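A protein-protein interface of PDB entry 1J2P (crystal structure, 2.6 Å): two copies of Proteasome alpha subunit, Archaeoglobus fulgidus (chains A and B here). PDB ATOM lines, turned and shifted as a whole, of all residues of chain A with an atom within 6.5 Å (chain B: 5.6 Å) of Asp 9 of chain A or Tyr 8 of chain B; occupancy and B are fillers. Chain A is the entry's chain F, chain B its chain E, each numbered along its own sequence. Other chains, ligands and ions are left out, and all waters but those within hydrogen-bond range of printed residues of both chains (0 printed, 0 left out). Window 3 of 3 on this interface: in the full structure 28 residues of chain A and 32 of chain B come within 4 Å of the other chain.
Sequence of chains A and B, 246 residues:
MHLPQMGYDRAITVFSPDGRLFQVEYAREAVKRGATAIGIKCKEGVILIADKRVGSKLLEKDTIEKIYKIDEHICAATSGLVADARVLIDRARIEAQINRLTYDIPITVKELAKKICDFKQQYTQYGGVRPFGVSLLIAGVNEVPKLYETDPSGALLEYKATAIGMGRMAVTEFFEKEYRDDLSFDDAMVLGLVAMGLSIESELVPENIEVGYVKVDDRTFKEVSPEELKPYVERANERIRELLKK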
ATOM      1  N   GLN A   5      17.961  20.810  14.523  1.00  0.00           N
ATOM      2  CA  GLN A   5      16.551  20.892  14.168  1.00  0.00           C
ATOM      3  C   GLN A   5      16.251  20.281  12.799  1.00  0.00           C
ATOM      4  O   GLN A   5      16.815  20.689  11.772  1.00  0.00           O
ATOM      5  CB  GLN A   5      16.081  22.351  14.200  1.00  0.00           C
ATOM      6  CG  GLN A   5      14.567  22.512  14.189  1.00  0.00           C
ATOM      7  CD  GLN A   5      13.906  21.974  15.455  1.00  0.00           C
ATOM      8  N   MET A   6      15.355  19.294  12.798  1.00  0.00           N
ATOM      9  CA  MET A   6      14.956  18.616  11.568  1.00  0.00           C
ATOM     10  C   MET A   6      14.494  19.684  10.578  1.00  0.00           C
ATOM     11  O   MET A   6      14.040  20.755  10.978  1.00  0.00           O
ATOM     12  CB  MET A   6      13.807  17.634  11.837  1.00  0.00           C
ATOM     13  N   GLY A   7      14.606  19.388   9.291  1.00  0.00           N
ATOM     14  CA  GLY A   7      14.199  20.355   8.295  1.00  0.00           C
ATOM     15  C   GLY A   7      15.378  21.126   7.743  1.00  0.00           C
ATOM     16  O   GLY A   7      15.337  21.581   6.606  1.00  0.00           O
ATOM     17  N   TYR A   8      16.435  21.271   8.537  1.00  0.00           N
ATOM     18  CA  TYR A   8      17.619  22.003   8.092  1.00  0.00           C
ATOM     19  C   TYR A   8      18.907  21.193   8.270  1.00  0.00           C
ATOM     20  O   TYR A   8      19.994  21.684   7.973  1.00  0.00           O
ATOM     21  CB  TYR A   8      17.755  23.302   8.890  1.00  0.00           C
ATOM     22  CG  TYR A   8      16.529  24.184   8.864  1.00  0.00           C
ATOM     23  CD1 TYR A   8      16.310  25.086   7.819  1.00  0.00           C
ATOM     24  CD2 TYR A   8      15.567  24.096   9.874  1.00  0.00           C
ATOM     25  CE1 TYR A   8      15.173  25.874   7.775  1.00  0.00           C
ATOM     26  CE2 TYR A   8      14.416  24.881   9.838  1.00  0.00           C
ATOM     27  CZ  TYR A   8      14.224  25.766   8.787  1.00  0.00           C
ATOM     28  OH  TYR A   8      13.074  26.521   8.744  1.00  0.00           O
ATOM     29  N   ASP A   9      18.792  19.950   8.725  1.00  0.00           N
ATOM     30  CA  ASP A   9      19.984  19.159   8.996  1.00  0.00           C
ATOM     31  C   ASP A   9      20.318  17.962   8.101  1.00  0.00           C
ATOM     32  O   ASP A   9      21.120  17.105   8.488  1.00  0.00           O
ATOM     33  CB  ASP A   9      19.945  18.696  10.458  1.00  0.00           C
ATOM     34  CG  ASP A   9      18.894  17.616  10.708  1.00  0.00           C
ATOM     35  OD1 ASP A   9      17.983  17.447   9.872  1.00  0.00           O
ATOM     36  OD2 ASP A   9      18.979  16.944  11.749  1.00  0.00           O
ATOM     37  N   ARG A  10      19.728  17.872   6.917  1.00  0.00           N
ATOM     38  CA  ARG A  10      20.079  16.742   6.076  1.00  0.00           C
ATOM     39  C   ARG A  10      20.576  17.094   4.680  1.00  0.00           C
ATOM     40  O   ARG A  10      20.467  16.300   3.755  1.00  0.00           O
ATOM     41  CB  ARG A  10      18.929  15.732   6.024  1.00  0.00           C
ATOM     42  CG  ARG A  10      17.564  16.292   5.754  1.00  0.00           C
ATOM     43  CD  ARG A  10      16.514  15.230   6.075  1.00  0.00           C
ATOM     44  NE  ARG A  10      15.201  15.553   5.518  1.00  0.00           N
ATOM     45  CZ  ARG A  10      14.134  14.765   5.618  1.00  0.00           C
ATOM     46  NH1 ARG A  10      12.973  15.133   5.080  1.00  0.00           N
ATOM     47  NH2 ARG A  10      14.225  13.604   6.256  1.00  0.00           N
ATOM     48  N   ALA A  11      21.151  18.286   4.547  1.00  0.00           N
ATOM     49  CA  ALA A  11      21.709  18.759   3.278  1.00  0.00           C
ATOM     50  C   ALA A  11      22.831  19.743   3.615  1.00  0.00           C
ATOM     51  O   ALA A  11      22.583  20.837   4.122  1.00  0.00           O
ATOM     52  CB  ALA A  11      20.630  19.443   2.432  1.00  0.00           C
ATOM     53  N   ILE A  12      24.059  19.341   3.317  1.00  0.00           N
ATOM     54  CA  ILE A  12      25.244  20.142   3.607  1.00  0.00           C
ATOM     55  C   ILE A  12      25.188  21.594   3.134  1.00  0.00           C
ATOM     56  O   ILE A  12      25.796  22.482   3.735  1.00  0.00           O
ATOM     57  CB  ILE A  12      26.516  19.477   3.010  1.00  0.00           C
ATOM     58  CG1 ILE A  12      27.763  20.240   3.447  1.00  0.00           C
ATOM     59  CG2 ILE A  12      26.426  19.450   1.495  1.00  0.00           C
ATOM     60  CD1 ILE A  12      27.937  20.313   4.943  1.00  0.00           C
ATOM     61  N   VAL A  14      22.549  23.556   3.094  1.00  0.00           N
ATOM     62  CA  VAL A  14      21.517  24.360   3.734  1.00  0.00           C
ATOM     63  C   VAL A  14      21.912  24.930   5.086  1.00  0.00           C
ATOM     64  O   VAL A  14      22.392  24.206   5.956  1.00  0.00           O
ATOM     65  CB  VAL A  14      20.223  23.535   3.901  1.00  0.00           C
ATOM     66  CG1 VAL A  14      19.190  24.307   4.704  1.00  0.00           C
ATOM     67  CG2 VAL A  14      19.666  23.189   2.549  1.00  0.00           C
ATOM     68  N   SER A  16      20.865  26.683   8.654  1.00  0.00           N
ATOM     69  CA  SER A  16      19.715  26.590   9.540  1.00  0.00           C
ATOM     70  C   SER A  16      19.309  28.044   9.819  1.00  0.00           C
ATOM     71  O   SER A  16      20.030  28.969   9.456  1.00  0.00           O
ATOM     72  CB  SER A  16      20.115  25.898  10.845  1.00  0.00           C
ATOM     73  OG  SER A  16      21.110  26.666  11.515  1.00  0.00           O
ATOM     74  N   PHE A  22      24.440  22.017  10.052  1.00  0.00           N
ATOM     75  CA  PHE A  22      24.295  20.807  10.846  1.00  0.00           C
ATOM     76  C   PHE A  22      24.988  19.552  10.305  1.00  0.00           C
ATOM     77  O   PHE A  22      25.490  18.744  11.088  1.00  0.00           O
ATOM     78  CB  PHE A  22      22.812  20.544  11.128  1.00  0.00           C
ATOM     79  CG  PHE A  22      22.222  21.495  12.131  1.00  0.00           C
ATOM     80  CD1 PHE A  22      22.823  21.676  13.373  1.00  0.00           C
ATOM     81  CD2 PHE A  22      21.103  22.255  11.821  1.00  0.00           C
ATOM     82  CE1 PHE A  22      22.321  22.609  14.290  1.00  0.00           C
ATOM     83  CE2 PHE A  22      20.594  23.183  12.726  1.00  0.00           C
ATOM     84  CZ  PHE A  22      21.206  23.363  13.960  1.00  0.00           C
ATOM     85  N   GLN A  23      25.043  19.383   8.986  1.00  0.00           N
ATOM     86  CA  GLN A  23      25.722  18.211   8.447  1.00  0.00           C
ATOM     87  C   GLN A  23      27.217  18.236   8.806  1.00  0.00           C
ATOM     88  O   GLN A  23      27.852  17.192   8.953  1.00  0.00           O
ATOM     89  CB  GLN A  23      25.510  18.097   6.935  1.00  0.00           C
ATOM     90  CG  GLN A  23      24.225  17.326   6.551  1.00  0.00           C
ATOM     91  CD  GLN A  23      24.207  15.866   7.046  1.00  0.00           C
ATOM     92  OE1 GLN A  23      23.406  15.493   7.920  1.00  0.00           O
ATOM     93  NE2 GLN A  23      25.090  15.040   6.488  1.00  0.00           N
ATOM     94  N   TYR A  26      27.311  17.244  12.460  1.00  0.00           N
ATOM     95  CA  TYR A  26      27.082  15.813  12.563  1.00  0.00           C
ATOM     96  C   TYR A  26      28.349  15.076  12.153  1.00  0.00           C
ATOM     97  O   TYR A  26      28.712  14.070  12.758  1.00  0.00           O
ATOM     98  CB  TYR A  26      25.915  15.395  11.679  1.00  0.00           C
ATOM     99  CG  TYR A  26      24.559  15.881  12.166  1.00  0.00           C
ATOM    100  CD1 TYR A  26      24.432  16.622  13.350  1.00  0.00           C
ATOM    101  CD2 TYR A  26      23.400  15.599  11.439  1.00  0.00           C
ATOM    102  CE1 TYR A  26      23.186  17.065  13.789  1.00  0.00           C
ATOM    103  CE2 TYR A  26      22.152  16.039  11.870  1.00  0.00           C
ATOM    104  CZ  TYR A  26      22.052  16.766  13.043  1.00  0.00           C
ATOM    105  OH  TYR A  26      20.811  17.166  13.473  1.00  0.00           O
ATOM    106  N   GLN B   5      17.740   5.432  12.262  1.00  0.00           N
ATOM    107  CA  GLN B   5      16.641   6.389  12.362  1.00  0.00           C
ATOM    108  C   GLN B   5      16.220   6.947  11.006  1.00  0.00           C
ATOM    109  O   GLN B   5      17.028   7.529  10.273  1.00  0.00           O
ATOM    110  CB  GLN B   5      17.024   7.538  13.303  1.00  0.00           C
ATOM    111  CG  GLN B   5      15.844   8.386  13.753  1.00  0.00           C
ATOM    112  CD  GLN B   5      14.864   7.616  14.633  1.00  0.00           C
ATOM    113  N   MET B   6      14.943   6.757  10.682  1.00  0.00           N
ATOM    114  CA  MET B   6      14.382   7.240   9.426  1.00  0.00           C
ATOM    115  C   MET B   6      14.674   8.737   9.334  1.00  0.00           C
ATOM    116  O   MET B   6      14.811   9.413  10.355  1.00  0.00           O
ATOM    117  CB  MET B   6      12.866   7.013   9.387  1.00  0.00           C
ATOM    118  N   GLY B   7      14.769   9.248   8.114  1.00  0.00           N
ATOM    119  CA  GLY B   7      15.052  10.658   7.942  1.00  0.00           C
ATOM    120  C   GLY B   7      16.517  10.901   7.645  1.00  0.00           C
ATOM    121  O   GLY B   7      16.861  11.884   7.001  1.00  0.00           O
ATOM    122  N   TYR B   8      17.382  10.005   8.108  1.00  0.00           N
ATOM    123  CA  TYR B   8      18.818  10.146   7.875  1.00  0.00           C
ATOM    124  C   TYR B   8      19.431   8.884   7.263  1.00  0.00           C
ATOM    125  O   TYR B   8      20.642   8.833   7.045  1.00  0.00           O
ATOM    126  CB  TYR B   8      19.545  10.434   9.193  1.00  0.00           C
ATOM    127  CG  TYR B   8      19.010  11.616   9.961  1.00  0.00           C
ATOM    128  CD1 TYR B   8      19.438  12.918   9.675  1.00  0.00           C
ATOM    129  CD2 TYR B   8      18.046  11.441  10.966  1.00  0.00           C
ATOM    130  CE1 TYR B   8      18.924  14.009  10.363  1.00  0.00           C
ATOM    131  CE2 TYR B   8      17.528  12.526  11.657  1.00  0.00           C
ATOM    132  CZ  TYR B   8      17.965  13.807  11.354  1.00  0.00           C
ATOM    133  OH  TYR B   8      17.436  14.878  12.024  1.00  0.00           O
ATOM    134  N   ASP B   9      18.612   7.880   6.961  1.00  0.00           N
ATOM    135  CA  ASP B   9      19.152   6.632   6.441  1.00  0.00           C
ATOM    136  C   ASP B   9      18.884   6.229   4.993  1.00  0.00           C
ATOM    137  O   ASP B   9      19.032   5.057   4.649  1.00  0.00           O
ATOM    138  CB  ASP B   9      18.719   5.482   7.348  1.00  0.00           C
ATOM    139  CG  ASP B   9      17.241   5.158   7.218  1.00  0.00           C
ATOM    140  OD1 ASP B   9      16.476   5.997   6.705  1.00  0.00           O
ATOM    141  OD2 ASP B   9      16.848   4.060   7.649  1.00  0.00           O
ATOM    142  N   ARG B  10      18.494   7.162   4.134  1.00  0.00           N
ATOM    143  CA  ARG B  10      18.273   6.769   2.758  1.00  0.00           C
ATOM    144  C   ARG B  10      19.028   7.579   1.716  1.00  0.00           C
ATOM    145  O   ARG B  10      18.605   7.689   0.566  1.00  0.00           O
ATOM    146  CB  ARG B  10      16.774   6.716   2.449  1.00  0.00           C
ATOM    147  CG  ARG B  10      15.969   7.897   2.876  1.00  0.00           C
ATOM    148  CD  ARG B  10      14.482   7.532   2.811  1.00  0.00           C
ATOM    149  NE  ARG B  10      13.619   8.711   2.854  1.00  0.00           N
ATOM    150  CZ  ARG B  10      12.296   8.670   2.749  1.00  0.00           C
ATOM    151  NH1 ARG B  10      11.591   9.794   2.798  1.00  0.00           N
ATOM    152  NH2 ARG B  10      11.677   7.505   2.599  1.00  0.00           N
ATOM    153  N   ALA B  11      20.163   8.129   2.124  1.00  0.00           N
ATOM    154  CA  ALA B  11      21.037   8.908   1.241  1.00  0.00           C
ATOM    155  C   ALA B  11      22.475   8.783   1.774  1.00  0.00           C
ATOM    156  O   ALA B  11      22.804   9.300   2.838  1.00  0.00           O
ATOM    157  CB  ALA B  11      20.600  10.367   1.204  1.00  0.00           C
ATOM    158  N   VAL B  14      24.354  11.650   3.523  1.00  0.00           N
ATOM    159  CA  VAL B  14      23.843  12.292   4.725  1.00  0.00           C
ATOM    160  C   VAL B  14      24.325  11.670   6.033  1.00  0.00           C
ATOM    161  O   VAL B  14      24.253  10.465   6.233  1.00  0.00           O
ATOM    162  CB  VAL B  14      22.298  12.318   4.706  1.00  0.00           C
ATOM    163  CG1 VAL B  14      21.747  12.855   6.030  1.00  0.00           C
ATOM    164  CG2 VAL B  14      21.819  13.174   3.542  1.00  0.00           C
ATOM    165  N   PHE B  15      24.854  12.512   6.907  1.00  0.00           N
ATOM    166  CA  PHE B  15      25.288  12.073   8.216  1.00  0.00           C
ATOM    167  C   PHE B  15      24.044  12.120   9.107  1.00  0.00           C
ATOM    168  O   PHE B  15      23.157  12.954   8.904  1.00  0.00           O
ATOM    169  CB  PHE B  15      26.320  13.041   8.792  1.00  0.00           C
ATOM    170  CG  PHE B  15      27.716  12.788   8.336  1.00  0.00           C
ATOM    171  CD1 PHE B  15      28.482  11.782   8.930  1.00  0.00           C
ATOM    172  CD2 PHE B  15      28.290  13.578   7.330  1.00  0.00           C
ATOM    173  CE1 PHE B  15      29.803  11.569   8.536  1.00  0.00           C
ATOM    174  CE2 PHE B  15      29.600  13.375   6.930  1.00  0.00           C
ATOM    175  CZ  PHE B  15      30.369  12.365   7.536  1.00  0.00           C
ATOM    176  N   SER B  16      23.993  11.236  10.091  1.00  0.00           N
ATOM    177  CA  SER B  16      22.891  11.204  11.037  1.00  0.00           C
ATOM    178  C   SER B  16      23.290  12.162  12.167  1.00  0.00           C
ATOM    179  O   SER B  16      24.435  12.604  12.231  1.00  0.00           O
ATOM    180  CB  SER B  16      22.711   9.788  11.582  1.00  0.00           C
ATOM    181  OG  SER B  16      23.868   9.372  12.289  1.00  0.00           O
ATOM    182  N   PRO B  17      22.353  12.491  13.072  1.00  0.00           N
ATOM    183  CA  PRO B  17      22.716  13.404  14.156  1.00  0.00           C
ATOM    184  C   PRO B  17      23.865  12.890  15.023  1.00  0.00           C
ATOM    185  O   PRO B  17      24.589  13.670  15.624  1.00  0.00           O
ATOM    186  CB  PRO B  17      21.408  13.559  14.925  1.00  0.00           C
ATOM    187  CG  PRO B  17      20.386  13.464  13.846  1.00  0.00           C
ATOM    188  CD  PRO B  17      20.895  12.273  13.048  1.00  0.00           C
ATOM    189  N   ARG B  20      26.786   9.230  11.743  1.00  0.00           N
ATOM    190  CA  ARG B  20      26.903   7.950  11.081  1.00  0.00           C
ATOM    191  C   ARG B  20      26.410   8.002   9.639  1.00  0.00           C
ATOM    192  O   ARG B  20      25.755   8.949   9.221  1.00  0.00           O
ATOM    193  CB  ARG B  20      26.148   6.891  11.890  1.00  0.00           C
ATOM    194  CG  ARG B  20      26.749   6.685  13.279  1.00  0.00           C
ATOM    195  CD  ARG B  20      25.767   6.059  14.249  1.00  0.00           C
ATOM    196  NE  ARG B  20      25.492   4.658  13.951  1.00  0.00           N
ATOM    197  CZ  ARG B  20      24.623   3.906  14.625  1.00  0.00           C
ATOM    198  NH1 ARG B  20      23.944   4.424  15.640  1.00  0.00           N
ATOM    199  NH2 ARG B  20      24.426   2.640  14.280  1.00  0.00           N
ATOM    200  N   PHE B  22      24.316   5.642   7.778  1.00  0.00           N
ATOM    201  CA  PHE B  22      23.459   4.473   7.788  1.00  0.00           C
ATOM    202  C   PHE B  22      23.429   3.653   6.495  1.00  0.00           C
ATOM    203  O   PHE B  22      23.320   2.425   6.555  1.00  0.00           O
ATOM    204  CB  PHE B  22      22.041   4.864   8.225  1.00  0.00           C
ATOM    205  CG  PHE B  22      21.939   5.180   9.690  1.00  0.00           C
ATOM    206  CD1 PHE B  22      22.401   4.274  10.640  1.00  0.00           C
ATOM    207  CD2 PHE B  22      21.447   6.407  10.128  1.00  0.00           C
ATOM    208  CE1 PHE B  22      22.387   4.588  12.006  1.00  0.00           C
ATOM    209  CE2 PHE B  22      21.429   6.728  11.487  1.00  0.00           C
ATOM    210  CZ  PHE B  22      21.904   5.814  12.421  1.00  0.00           C
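The backbone carbonyl oxygen (O) of Gly 7 of chain B is in hydrogen-bond range of the guanidinium group (NH2) of Arg 10 of chain A (3.2 Å).
The side-chain carboxylate (OD2) of Asp 9 of chain A is in hydrogen-bond range of the side-chain hydroxyl (OH) of Tyr 8 of chain B (2.6 Å).
The backbone NH (N) of Phe 15 of chain B lies close to the side-chain amide nitrogen (NE2) of Gln 23 of chain A (2.6 Å).
The backbone NH (N) of Arg 20 of chain B is in hydrogen-bond range of the side-chain hydroxyl (OG) of Ser 16 of chain B.
The backbone carbonyl oxygen (O) of Asp 9 of chain A sits close to the side-chain amide oxygen (OE1) of Gln 23 of chain A.
The side-chain hydroxyl of Tyr 26 of chain A sits at hydrogen-bond distance from the side-chain carboxylate of Asp 9 of chain A.
O of Arg 10 of chain A touches CG2 of Val 14 of chain B (3.4 Å).
NE2 of Gln 23 of chain A touches C of Val 14 of chain B (3.5 Å).
Tyr 26 of chain A touches Phe 15 of chain B (CD2 to O, 3.7 Å).
Tyr 26 of chain A touches Ser 16 of chain B (CB to O, 3.2 Å).
CA of Pro 17 of chain B touches CE2 of Tyr 26 of chain A, 3.5 Å away.
Tyr 8 of chain A touches none of the printed residues of chain B.
Asp 9 of chain A touches just one residue of chain B: Tyr 8.
Ser 16 of chain A touches none of the printed residues of chain B.
Printed residues of chain B within 4 Å of Gln 23 of chain A: Val 14 and Phe 15.
Of chain A, only Asp 9 comes within 4 Å of Tyr 8 of chain B.
Printed residues of chain A within 4 Å of Val 14 of chain B: Arg 10 and Gln 23.
Of the printed residues of chain A, Ser 16 of chain B touches Tyr 26 (3.2 Å).
The nearest residue of chain B that does not touch Asp 9 of chain A is Pro 17 of chain B (4.3 Å).
The nearest residue of chain A that does not touch Tyr 8 of chain B is Tyr 26 of chain A (4.1 Å).
Of the 13 printed residues of chain B, 6 touch a printed residue of chain A.
Printed residues of chain A that touch a printed residue of chain B: Asp 9, Arg 10, Gln 23 and Tyr 26.
Among the printed residues, no Asp or Glu carboxylate lies within 4 Å of a Lys or Arg side-chain nitrogen of the other chain.
Asp 9 of chain A touches Tyr 8 of chain B, but with the chains exchanged Tyr 8 of chain A does not touch Asp 9 of chain B (13.4 Å).
Arg 10 of chain A touches Gly 7 of chain B, but with the chains exchanged Gly 7 of chain A does not touch Arg 10 of chain B (12.0 Å).
Arg 10 of chain A touches Val 14 of chain B, but with the chains exchanged Val 14 of chain A does not touch Arg 10 of chain B (15.6 Å).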
